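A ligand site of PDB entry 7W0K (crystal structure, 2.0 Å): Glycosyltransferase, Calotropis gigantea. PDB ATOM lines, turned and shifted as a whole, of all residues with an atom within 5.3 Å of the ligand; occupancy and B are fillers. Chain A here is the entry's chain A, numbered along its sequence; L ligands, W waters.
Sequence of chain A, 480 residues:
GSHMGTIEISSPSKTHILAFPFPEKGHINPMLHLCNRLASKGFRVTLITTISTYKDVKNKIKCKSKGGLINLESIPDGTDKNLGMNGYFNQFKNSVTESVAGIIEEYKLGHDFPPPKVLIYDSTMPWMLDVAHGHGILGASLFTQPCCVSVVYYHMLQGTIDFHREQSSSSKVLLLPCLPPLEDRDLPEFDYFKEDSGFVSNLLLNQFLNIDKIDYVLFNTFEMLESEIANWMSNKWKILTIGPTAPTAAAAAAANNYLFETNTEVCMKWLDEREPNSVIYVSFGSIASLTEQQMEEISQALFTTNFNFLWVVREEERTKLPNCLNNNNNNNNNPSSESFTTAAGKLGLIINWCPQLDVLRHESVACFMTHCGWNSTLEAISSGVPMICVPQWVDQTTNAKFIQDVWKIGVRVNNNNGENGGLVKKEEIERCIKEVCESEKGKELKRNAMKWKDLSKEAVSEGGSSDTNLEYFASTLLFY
N of Asn 375 sits at hydrogen-bond distance from O8 of the ligand, 3.0 Å away. An oxygen (O8) of the ligand is in hydrogen-bond range of the side-chain amide nitrogen of Asn 375 (2.8 Å). O of Cys 354 is in hydrogen-bond range of N2 of the ligand, 2.8 Å away. An oxygen (O2) of the ligand sits at hydrogen-bond distance from the backbone NH (N) of Cys 354 (3.0 Å). OE2 of Glu 261 sits close to O1 of the ligand, at 2.7 Å. The side-chain carboxylate of Glu 379 is in hydrogen-bond range of an oxygen (O3) of the ligand (2.7 Å). The side-chain hydroxyl of Ser 286 lies within hydrogen-bond range of an oxygen (O11) of the ligand (2.8 Å). OG of Ser 376 lies within hydrogen-bond range of O7 of the ligand. O11 of the ligand sits at hydrogen-bond distance from N of Ser 286 (2.9 Å). An oxygen (O8) of the ligand sits at hydrogen-bond distance from the backbone NH (N) of Trp 374, at 3.4 Å. The backbone NH of Ser 376 sits at hydrogen-bond distance from an oxygen (O7) of the ligand. The side-chain amide nitrogen of Asn 29 lies within hydrogen-bond range of an oxygen (O5) of the ligand (3.0 Å). An oxygen (O9) of the ligand sits at hydrogen-bond distance from a ring nitrogen (NE2) of His 371 (2.9 Å). The side-chain sulfur (SG) of Cys 354 is in hydrogen-bond range of an oxygen (O2) of the ligand, at 3.4 Å. The side-chain amide oxygen (OE1) of Gln 356 sits at hydrogen-bond distance from an oxygen (O3) of the ligand (3.2 Å).
The side-chain carboxylate (OE1) of Glu 379 sits close to the side-chain amide oxygen (OE1) of Gln 356 (3.0 Å). The backbone NH (N) of His 371 lies within hydrogen-bond range of the backbone carbonyl oxygen (O) of Ser 283, at 3.5 Å. The backbone NH (N) of Gln 356 lies close to the side-chain sulfur (SG) of Cys 354 (3.7 Å). The side-chain hydroxyl (OG) of Ser 376 sits at hydrogen-bond distance from the side-chain amide oxygen (OE1) of Gln 356, at 3.1 Å. O of Gly 373 is in hydrogen-bond range of OG1 of Thr 377 (3.0 Å). The side-chain hydroxyl of Ser 283 sits at hydrogen-bond distance from the backbone NH of Gly 285 (3.2 Å). The backbone carbonyl oxygen (O) of Gly 26 lies within hydrogen-bond range of the side-chain amide nitrogen (ND2) of Asn 375 (2.6 Å). The side-chain sulfur (SG) of Cys 354 sits at hydrogen-bond distance from the side-chain hydroxyl (OH) of Tyr 281, 3.2 Å away.
NE1 of Trp 353 lies close to N2 of the ligand, at 3.4 Å. CA of Gly 26 touches O6 of the ligand, 3.5 Å away. Tyr 281 touches the ligand (OH to O2, 3.8 Å). OG of Ser 283 touches C3 of the ligand, 3.6 Å away. Gly 285 touches the ligand (CA to O11, 3.8 Å). Val 312 touches the ligand. Gly 373 touches the ligand. Hydrophobic or aromatic side chains within 4 Å of the ligand: Val 312, Trp 353 and His 371. Along chain A the residues within 4 Å of the ligand span positions 26 to 379.
Water W2 lies within hydrogen-bond range of the backbone NH (N) of Ala 288 (2.6 Å), an oxygen (O10) of the ligand (2.6 Å), the backbone NH (N) of Ile 287 (2.9 Å) and the backbone carbonyl oxygen (O) of Phe 284 (2.9 Å). Water W3 lies within hydrogen-bond range of the side-chain amide nitrogen (NE2) of Gln 356 (2.5 Å), the side-chain hydroxyl (OG) of Ser 283 (2.8 Å) and the side-chain hydroxyl (OG) of Ser 376 (3.1 Å). Water W4 lies within hydrogen-bond range of OE2 of Glu 379 and O5 of the ligand.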
ATOM      1  N   LYS A  25     -27.161 -15.814  10.009  1.00  0.00           N
ATOM      2  CA  LYS A  25     -27.389 -14.682   9.111  1.00  0.00           C
ATOM      3  C   LYS A  25     -26.127 -13.853   8.907  1.00  0.00           C
ATOM      4  O   LYS A  25     -25.896 -13.341   7.815  1.00  0.00           O
ATOM      5  CB  LYS A  25     -28.512 -13.799   9.643  1.00  0.00           C
ATOM      6  CG  LYS A  25     -29.839 -14.533   9.800  1.00  0.00           C
ATOM      7  CD  LYS A  25     -30.980 -13.701   9.258  1.00  0.00           C
ATOM      8  CE  LYS A  25     -32.192 -14.575   9.025  1.00  0.00           C
ATOM      9  NZ  LYS A  25     -32.377 -15.480  10.184  1.00  0.00           N
ATOM     10  N   GLY A  26     -25.318 -13.697   9.952  1.00  0.00           N
ATOM     11  CA  GLY A  26     -24.045 -12.989   9.841  1.00  0.00           C
ATOM     12  C   GLY A  26     -23.014 -13.695   8.989  1.00  0.00           C
ATOM     13  O   GLY A  26     -21.953 -13.127   8.699  1.00  0.00           O
ATOM     14  N   ASN A  29     -25.391 -13.776   4.957  1.00  0.00           N
ATOM     15  CA  ASN A  29     -25.560 -12.514   4.241  1.00  0.00           C
ATOM     16  C   ASN A  29     -24.312 -12.061   3.500  1.00  0.00           C
ATOM     17  O   ASN A  29     -24.434 -11.690   2.317  1.00  0.00           O
ATOM     18  CB  ASN A  29     -26.049 -11.431   5.199  1.00  0.00           C
ATOM     19  CG  ASN A  29     -27.502 -11.606   5.566  1.00  0.00           C
ATOM     20  OD1 ASN A  29     -28.170 -12.500   5.068  1.00  0.00           O
ATOM     21  ND2 ASN A  29     -27.984 -10.750   6.470  1.00  0.00           N
ATOM     22  N   GLU A 261     -35.049  -8.232   2.125  1.00  0.00           N
ATOM     23  CA  GLU A 261     -35.416  -8.700   3.451  1.00  0.00           C
ATOM     24  C   GLU A 261     -36.869  -8.337   3.759  1.00  0.00           C
ATOM     25  O   GLU A 261     -37.480  -7.494   3.098  1.00  0.00           O
ATOM     26  CB  GLU A 261     -34.475  -8.151   4.530  1.00  0.00           C
ATOM     27  CG  GLU A 261     -33.027  -8.729   4.505  1.00  0.00           C
ATOM     28  CD  GLU A 261     -32.792  -9.849   5.512  1.00  0.00           C
ATOM     29  OE1 GLU A 261     -33.746 -10.607   5.828  1.00  0.00           O
ATOM     30  OE2 GLU A 261     -31.631  -9.999   5.990  1.00  0.00           O
ATOM     31  N   TYR A 281     -31.637   3.958  15.013  1.00  0.00           N
ATOM     32  CA  TYR A 281     -31.883   2.578  14.629  1.00  0.00           C
ATOM     33  C   TYR A 281     -31.166   1.674  15.628  1.00  0.00           C
ATOM     34  O   TYR A 281     -29.969   1.874  15.880  1.00  0.00           O
ATOM     35  CB  TYR A 281     -31.387   2.293  13.210  1.00  0.00           C
ATOM     36  CG  TYR A 281     -31.412   0.818  12.840  1.00  0.00           C
ATOM     37  CD1 TYR A 281     -32.588   0.083  12.899  1.00  0.00           C
ATOM     38  CD2 TYR A 281     -30.240   0.156  12.463  1.00  0.00           C
ATOM     39  CE1 TYR A 281     -32.608  -1.275  12.586  1.00  0.00           C
ATOM     40  CE2 TYR A 281     -30.255  -1.199  12.134  1.00  0.00           C
ATOM     41  CZ  TYR A 281     -31.442  -1.908  12.196  1.00  0.00           C
ATOM     42  OH  TYR A 281     -31.439  -3.249  11.869  1.00  0.00           O
ATOM     43  N   SER A 283     -30.469  -2.376  16.847  1.00  0.00           N
ATOM     44  CA  SER A 283     -30.533  -3.799  16.562  1.00  0.00           C
ATOM     45  C   SER A 283     -29.338  -4.493  17.200  1.00  0.00           C
ATOM     46  O   SER A 283     -28.234  -3.961  17.222  1.00  0.00           O
ATOM     47  CB  SER A 283     -30.550  -4.073  15.058  1.00  0.00           C
ATOM     48  OG  SER A 283     -30.458  -5.466  14.807  1.00  0.00           O
ATOM     49  N   PHE A 284     -29.583  -5.698  17.741  1.00  0.00           N
ATOM     50  CA  PHE A 284     -28.519  -6.489  18.337  1.00  0.00           C
ATOM     51  C   PHE A 284     -28.271  -7.753  17.527  1.00  0.00           C
ATOM     52  O   PHE A 284     -27.702  -8.716  18.039  1.00  0.00           O
ATOM     53  CB  PHE A 284     -28.853  -6.801  19.794  1.00  0.00           C
ATOM     54  CG  PHE A 284     -28.699  -5.604  20.694  1.00  0.00           C
ATOM     55  CD1 PHE A 284     -29.706  -4.651  20.784  1.00  0.00           C
ATOM     56  CD2 PHE A 284     -27.521  -5.385  21.382  1.00  0.00           C
ATOM     57  CE1 PHE A 284     -29.552  -3.527  21.588  1.00  0.00           C
ATOM     58  CE2 PHE A 284     -27.354  -4.241  22.182  1.00  0.00           C
ATOM     59  CZ  PHE A 284     -28.369  -3.321  22.274  1.00  0.00           C
ATOM     60  N   GLY A 285     -28.659  -7.729  16.263  1.00  0.00           N
ATOM     61  CA  GLY A 285     -28.347  -8.779  15.322  1.00  0.00           C
ATOM     62  C   GLY A 285     -29.329  -9.930  15.396  1.00  0.00           C
ATOM     63  O   GLY A 285     -30.414  -9.850  15.982  1.00  0.00           O
ATOM     64  N   SER A 286     -28.902 -11.037  14.789  1.00  0.00           N
ATOM     65  CA  SER A 286     -29.720 -12.214  14.561  1.00  0.00           C
ATOM     66  C   SER A 286     -29.578 -13.263  15.648  1.00  0.00           C
ATOM     67  O   SER A 286     -30.401 -14.186  15.702  1.00  0.00           O
ATOM     68  CB  SER A 286     -29.333 -12.842  13.212  1.00  0.00           C
ATOM     69  OG  SER A 286     -28.088 -13.493  13.309  1.00  0.00           O
ATOM     70  N   ILE A 287     -28.577 -13.148  16.538  1.00  0.00           N
ATOM     71  CA  ILE A 287     -28.220 -14.213  17.464  1.00  0.00           C
ATOM     72  C   ILE A 287     -28.247 -13.753  18.923  1.00  0.00           C
ATOM     73  O   ILE A 287     -28.708 -14.500  19.797  1.00  0.00           O
ATOM     74  CB  ILE A 287     -26.828 -14.780  17.093  1.00  0.00           C
ATOM     75  CG1 ILE A 287     -26.972 -15.878  16.027  1.00  0.00           C
ATOM     76  CG2 ILE A 287     -26.158 -15.406  18.299  1.00  0.00           C
ATOM     77  CD1 ILE A 287     -27.739 -17.097  16.529  1.00  0.00           C
ATOM     78  N   ALA A 288     -27.757 -12.552  19.209  1.00  0.00           N
ATOM     79  CA  ALA A 288     -27.621 -12.130  20.602  1.00  0.00           C
ATOM     80  C   ALA A 288     -28.990 -12.036  21.269  1.00  0.00           C
ATOM     81  O   ALA A 288     -29.991 -11.703  20.639  1.00  0.00           O
ATOM     82  CB  ALA A 288     -26.893 -10.805  20.697  1.00  0.00           C
ATOM     83  N   VAL A 312     -35.242  -3.229  16.366  1.00  0.00           N
ATOM     84  CA  VAL A 312     -35.475  -4.622  16.008  1.00  0.00           C
ATOM     85  C   VAL A 312     -35.373  -5.471  17.264  1.00  0.00           C
ATOM     86  O   VAL A 312     -34.331  -5.512  17.934  1.00  0.00           O
ATOM     87  CB  VAL A 312     -34.502  -5.104  14.930  1.00  0.00           C
ATOM     88  CG1 VAL A 312     -34.761  -6.565  14.617  1.00  0.00           C
ATOM     89  CG2 VAL A 312     -34.608  -4.249  13.668  1.00  0.00           C
ATOM     90  N   ASN A 352     -39.980  -7.034  14.245  1.00  0.00           N
ATOM     91  CA  ASN A 352     -39.267  -8.294  14.438  1.00  0.00           C
ATOM     92  C   ASN A 352     -38.024  -8.373  13.566  1.00  0.00           C
ATOM     93  O   ASN A 352     -37.081  -9.095  13.896  1.00  0.00           O
ATOM     94  CB  ASN A 352     -40.210  -9.480  14.159  1.00  0.00           C
ATOM     95  N   TRP A 353     -38.008  -7.656  12.444  1.00  0.00           N
ATOM     96  CA  TRP A 353     -36.906  -7.715  11.468  1.00  0.00           C
ATOM     97  C   TRP A 353     -37.097  -6.594  10.461  1.00  0.00           C
ATOM     98  O   TRP A 353     -38.225  -6.169  10.196  1.00  0.00           O
ATOM     99  CB  TRP A 353     -36.882  -9.072  10.756  1.00  0.00           C
ATOM    100  CG  TRP A 353     -35.551  -9.442  10.116  1.00  0.00           C
ATOM    101  CD1 TRP A 353     -35.277  -9.523   8.788  1.00  0.00           C
ATOM    102  CD2 TRP A 353     -34.344  -9.796  10.801  1.00  0.00           C
ATOM    103  NE1 TRP A 353     -33.970  -9.907   8.599  1.00  0.00           N
ATOM    104  CE2 TRP A 353     -33.383 -10.095   9.817  1.00  0.00           C
ATOM    105  CE3 TRP A 353     -33.987  -9.895  12.157  1.00  0.00           C
ATOM    106  CZ2 TRP A 353     -32.079 -10.470  10.139  1.00  0.00           C
ATOM    107  CZ3 TRP A 353     -32.696 -10.273  12.468  1.00  0.00           C
ATOM    108  CH2 TRP A 353     -31.757 -10.563  11.460  1.00  0.00           C
ATOM    109  N   CYS A 354     -35.986  -6.137   9.897  1.00  0.00           N
ATOM    110  CA  CYS A 354     -36.021  -5.026   8.946  1.00  0.00           C
ATOM    111  C   CYS A 354     -34.997  -5.225   7.823  1.00  0.00           C
ATOM    112  O   CYS A 354     -34.157  -6.124   7.919  1.00  0.00           O
ATOM    113  CB  CYS A 354     -35.781  -3.702   9.672  1.00  0.00           C
ATOM    114  SG  CYS A 354     -34.062  -3.336  10.015  1.00  0.00           S
ATOM    115  N   PRO A 355     -35.065  -4.437   6.742  1.00  0.00           N
ATOM    116  CA  PRO A 355     -33.964  -4.460   5.773  1.00  0.00           C
ATOM    117  C   PRO A 355     -32.850  -3.538   6.266  1.00  0.00           C
ATOM    118  O   PRO A 355     -32.815  -2.350   5.930  1.00  0.00           O
ATOM    119  CB  PRO A 355     -34.611  -3.952   4.486  1.00  0.00           C
ATOM    120  CG  PRO A 355     -35.677  -3.001   5.000  1.00  0.00           C
ATOM    121  CD  PRO A 355     -36.179  -3.576   6.294  1.00  0.00           C
ATOM    122  N   GLN A 356     -31.940  -4.097   7.065  1.00  0.00           N
ATOM    123  CA  GLN A 356     -31.008  -3.266   7.829  1.00  0.00           C
ATOM    124  C   GLN A 356     -30.211  -2.340   6.932  1.00  0.00           C
ATOM    125  O   GLN A 356     -30.012  -1.167   7.256  1.00  0.00           O
ATOM    126  CB  GLN A 356     -30.073  -4.145   8.657  1.00  0.00           C
ATOM    127  CG  GLN A 356     -28.950  -3.321   9.303  1.00  0.00           C
ATOM    128  CD  GLN A 356     -28.249  -4.039  10.418  1.00  0.00           C
ATOM    129  OE1 GLN A 356     -27.050  -4.323  10.336  1.00  0.00           O
ATOM    130  NE2 GLN A 356     -28.972  -4.327  11.477  1.00  0.00           N
ATOM    131  N   LEU A 357     -29.761  -2.821   5.764  1.00  0.00           N
ATOM    132  CA  LEU A 357     -28.963  -1.965   4.889  1.00  0.00           C
ATOM    133  C   LEU A 357     -29.792  -0.786   4.361  1.00  0.00           C
ATOM    134  O   LEU A 357     -29.301   0.348   4.307  1.00  0.00           O
ATOM    135  CB  LEU A 357     -28.356  -2.786   3.747  1.00  0.00           C
ATOM    136  CG  LEU A 357     -27.165  -2.171   2.995  1.00  0.00           C
ATOM    137  CD1 LEU A 357     -26.126  -1.632   3.940  1.00  0.00           C
ATOM    138  CD2 LEU A 357     -26.526  -3.173   2.013  1.00  0.00           C
ATOM    139  N   HIS A 371     -24.977  -4.118  18.414  1.00  0.00           N
ATOM    140  CA  HIS A 371     -24.131  -5.056  19.129  1.00  0.00           C
ATOM    141  C   HIS A 371     -22.732  -5.153  18.520  1.00  0.00           C
ATOM    142  O   HIS A 371     -21.870  -5.793  19.134  1.00  0.00           O
ATOM    143  CB  HIS A 371     -24.767  -6.447  19.177  1.00  0.00           C
ATOM    144  CG  HIS A 371     -24.701  -7.184  17.883  1.00  0.00           C
ATOM    145  ND1 HIS A 371     -25.029  -6.599  16.675  1.00  0.00           N
ATOM    146  CD2 HIS A 371     -24.352  -8.463  17.597  1.00  0.00           C
ATOM    147  CE1 HIS A 371     -24.881  -7.493  15.696  1.00  0.00           C
ATOM    148  NE2 HIS A 371     -24.469  -8.631  16.235  1.00  0.00           N
ATOM    149  N   GLY A 373     -21.713  -6.643  15.733  1.00  0.00           N
ATOM    150  CA  GLY A 373     -21.405  -7.754  14.845  1.00  0.00           C
ATOM    151  C   GLY A 373     -20.733  -7.198  13.602  1.00  0.00           C
ATOM    152  O   GLY A 373     -20.971  -6.035  13.262  1.00  0.00           O
ATOM    153  N   TRP A 374     -19.874  -7.980  12.930  1.00  0.00           N
ATOM    154  CA  TRP A 374     -19.048  -7.376  11.890  1.00  0.00           C
ATOM    155  C   TRP A 374     -19.885  -6.861  10.721  1.00  0.00           C
ATOM    156  O   TRP A 374     -19.602  -5.785  10.175  1.00  0.00           O
ATOM    157  CB  TRP A 374     -17.964  -8.336  11.385  1.00  0.00           C
ATOM    158  CG  TRP A 374     -17.138  -7.688  10.294  1.00  0.00           C
ATOM    159  CD1 TRP A 374     -16.940  -8.158   9.012  1.00  0.00           C
ATOM    160  CD2 TRP A 374     -16.443  -6.433  10.369  1.00  0.00           C
ATOM    161  NE1 TRP A 374     -16.147  -7.271   8.309  1.00  0.00           N
ATOM    162  CE2 TRP A 374     -15.830  -6.216   9.114  1.00  0.00           C
ATOM    163  CE3 TRP A 374     -16.281  -5.467  11.393  1.00  0.00           C
ATOM    164  CZ2 TRP A 374     -15.067  -5.080   8.857  1.00  0.00           C
ATOM    165  CZ3 TRP A 374     -15.522  -4.354  11.129  1.00  0.00           C
ATOM    166  CH2 TRP A 374     -14.926  -4.158   9.865  1.00  0.00           C
ATOM    167  N   ASN A 375     -20.903  -7.611  10.295  1.00  0.00           N
ATOM    168  CA  ASN A 375     -21.686  -7.162   9.145  1.00  0.00           C
ATOM    169  C   ASN A 375     -22.385  -5.856   9.458  1.00  0.00           C
ATOM    170  O   ASN A 375     -22.352  -4.904   8.664  1.00  0.00           O
ATOM    171  CB  ASN A 375     -22.695  -8.228   8.731  1.00  0.00           C
ATOM    172  CG  ASN A 375     -22.033  -9.477   8.193  1.00  0.00           C
ATOM    173  OD1 ASN A 375     -21.604  -9.505   7.039  1.00  0.00           O
ATOM    174  ND2 ASN A 375     -21.931 -10.512   9.027  1.00  0.00           N
ATOM    175  N   SER A 376     -23.026  -5.786  10.633  1.00  0.00           N
ATOM    176  CA  SER A 376     -23.633  -4.539  11.095  1.00  0.00           C
ATOM    177  C   SER A 376     -22.634  -3.392  11.105  1.00  0.00           C
ATOM    178  O   SER A 376     -22.944  -2.296  10.661  1.00  0.00           O
ATOM    179  CB  SER A 376     -24.196  -4.740  12.497  1.00  0.00           C
ATOM    180  OG  SER A 376     -25.235  -5.701  12.454  1.00  0.00           O
ATOM    181  N   THR A 377     -21.417  -3.644  11.595  1.00  0.00           N
ATOM    182  CA  THR A 377     -20.394  -2.591  11.635  1.00  0.00           C
ATOM    183  C   THR A 377     -20.044  -2.112  10.232  1.00  0.00           C
ATOM    184  O   THR A 377     -20.043  -0.913   9.951  1.00  0.00           O
ATOM    185  CB  THR A 377     -19.126  -3.107  12.346  1.00  0.00           C
ATOM    186  OG1 THR A 377     -19.415  -3.466  13.700  1.00  0.00           O
ATOM    187  CG2 THR A 377     -17.990  -2.036  12.336  1.00  0.00           C
ATOM    188  N   GLU A 379     -21.725  -2.622   7.354  1.00  0.00           N
ATOM    189  CA  GLU A 379     -22.863  -1.996   6.699  1.00  0.00           C
ATOM    190  C   GLU A 379     -23.023  -0.547   7.164  1.00  0.00           C
ATOM    191  O   GLU A 379     -23.270   0.350   6.338  1.00  0.00           O
ATOM    192  CB  GLU A 379     -24.141  -2.793   6.968  1.00  0.00           C
ATOM    193  CG  GLU A 379     -24.152  -4.144   6.223  1.00  0.00           C
ATOM    194  CD  GLU A 379     -25.100  -5.168   6.826  1.00  0.00           C
ATOM    195  OE1 GLU A 379     -25.979  -4.778   7.615  1.00  0.00           O
ATOM    196  OE2 GLU A 379     -24.950  -6.358   6.520  1.00  0.00           O
ATOM    197  N   TRP A 393     -20.430 -10.300  22.639  1.00  0.00           N
ATOM    198  CA  TRP A 393     -19.443 -11.373  22.800  1.00  0.00           C
ATOM    199  C   TRP A 393     -18.701 -11.585  21.475  1.00  0.00           C
ATOM    200  O   TRP A 393     -18.978 -10.907  20.481  1.00  0.00           O
ATOM    201  CB  TRP A 393     -20.096 -12.668  23.282  1.00  0.00           C
ATOM    202  CG  TRP A 393     -21.481 -12.827  22.799  1.00  0.00           C
ATOM    203  CD1 TRP A 393     -22.651 -12.705  23.530  1.00  0.00           C
ATOM    204  CD2 TRP A 393     -21.882 -13.133  21.465  1.00  0.00           C
ATOM    205  NE1 TRP A 393     -23.737 -12.920  22.711  1.00  0.00           N
ATOM    206  CE2 TRP A 393     -23.285 -13.177  21.439  1.00  0.00           C
ATOM    207  CE3 TRP A 393     -21.178 -13.367  20.278  1.00  0.00           C
ATOM    208  CZ2 TRP A 393     -24.003 -13.459  20.269  1.00  0.00           C
ATOM    209  CZ3 TRP A 393     -21.892 -13.650  19.122  1.00  0.00           C
ATOM    210  CH2 TRP A 393     -23.287 -13.687  19.131  1.00  0.00           C
ATOM    211  N   GLN A 396     -17.390  -8.762  18.763  1.00  0.00           N
ATOM    212  CA  GLN A 396     -18.085  -7.495  18.964  1.00  0.00           C
ATOM    213  C   GLN A 396     -17.307  -6.545  19.856  1.00  0.00           C
ATOM    214  O   GLN A 396     -17.303  -5.329  19.641  1.00  0.00           O
ATOM    215  CB  GLN A 396     -19.478  -7.764  19.549  1.00  0.00           C
ATOM    216  CG  GLN A 396     -20.398  -8.560  18.582  1.00  0.00           C
ATOM    217  CD  GLN A 396     -21.415  -9.453  19.280  1.00  0.00           C
ATOM    218  OE1 GLN A 396     -21.873  -9.148  20.376  1.00  0.00           O
ATOM    219  NE2 GLN A 396     -21.783 -10.545  18.624  1.00  0.00           N
HETATM  220  N1  LIG L   1     -30.090  -7.874   9.800  1.00  0.00           N
HETATM  221  C1  LIG L   1     -31.167  -7.649   9.074  1.00  0.00           C
HETATM  222  N2  LIG L   1     -32.266  -7.176   9.621  1.00  0.00           N
HETATM  223  C2  LIG L   1     -32.307  -6.892  10.914  1.00  0.00           C
HETATM  224  C3  LIG L   1     -31.196  -7.113  11.718  1.00  0.00           C
HETATM  225  C4  LIG L   1     -30.059  -7.624  11.100  1.00  0.00           C
HETATM  226  O1  LIG L   1     -31.170  -7.911   7.706  1.00  0.00           O
HETATM  227  O2  LIG L   1     -33.491  -6.404  11.457  1.00  0.00           O
HETATM  228  C5  LIG L   1     -28.880  -8.423   9.152  1.00  0.00           C
HETATM  229  C6  LIG L   1     -27.735  -7.426   9.221  1.00  0.00           C
HETATM  230  O3  LIG L   1     -27.891  -6.547   8.190  1.00  0.00           O
HETATM  231  C7  LIG L   1     -26.500  -8.363   9.128  1.00  0.00           C
HETATM  232  C8  LIG L   1     -26.857  -9.462   9.771  1.00  0.00           C
HETATM  233  O4  LIG L   1     -28.457  -9.438   9.850  1.00  0.00           O
HETATM  234  O5  LIG L   1     -26.128  -8.718   7.726  1.00  0.00           O
HETATM  235  C9  LIG L   1     -26.348  -9.461  11.205  1.00  0.00           C
HETATM  236  O6  LIG L   1     -25.014  -9.891  11.111  1.00  0.00           O
HETATM  237  P1  LIG L   1     -23.907  -9.348  12.176  1.00  0.00           P
HETATM  238  O7  LIG L   1     -24.023  -7.845  12.382  1.00  0.00           O
HETATM  239  O8  LIG L   1     -22.552  -9.714  11.654  1.00  0.00           O
HETATM  240  O9  LIG L   1     -24.148  -9.964  13.678  1.00  0.00           O
HETATM  241  P2  LIG L   1     -24.741 -11.427  14.097  1.00  0.00           P
HETATM  242  O10 LIG L   1     -24.500 -11.471  15.584  1.00  0.00           O
HETATM  243  O11 LIG L   1     -26.195 -11.506  13.754  1.00  0.00           O
HETATM  244  O12 LIG L   1     -23.936 -12.507  13.404  1.00  0.00           O
HETATM  245  O   HOH W   1     -29.819  -6.845   5.114  1.00  0.00           O
HETATM  246  O   HOH W   2     -26.487 -11.278  17.322  1.00  0.00           O
HETATM  247  O   HOH W   3     -28.239  -5.954  13.219  1.00  0.00           O
HETATM  248  O   HOH W   4     -27.012  -7.697   4.632  1.00  0.00           O
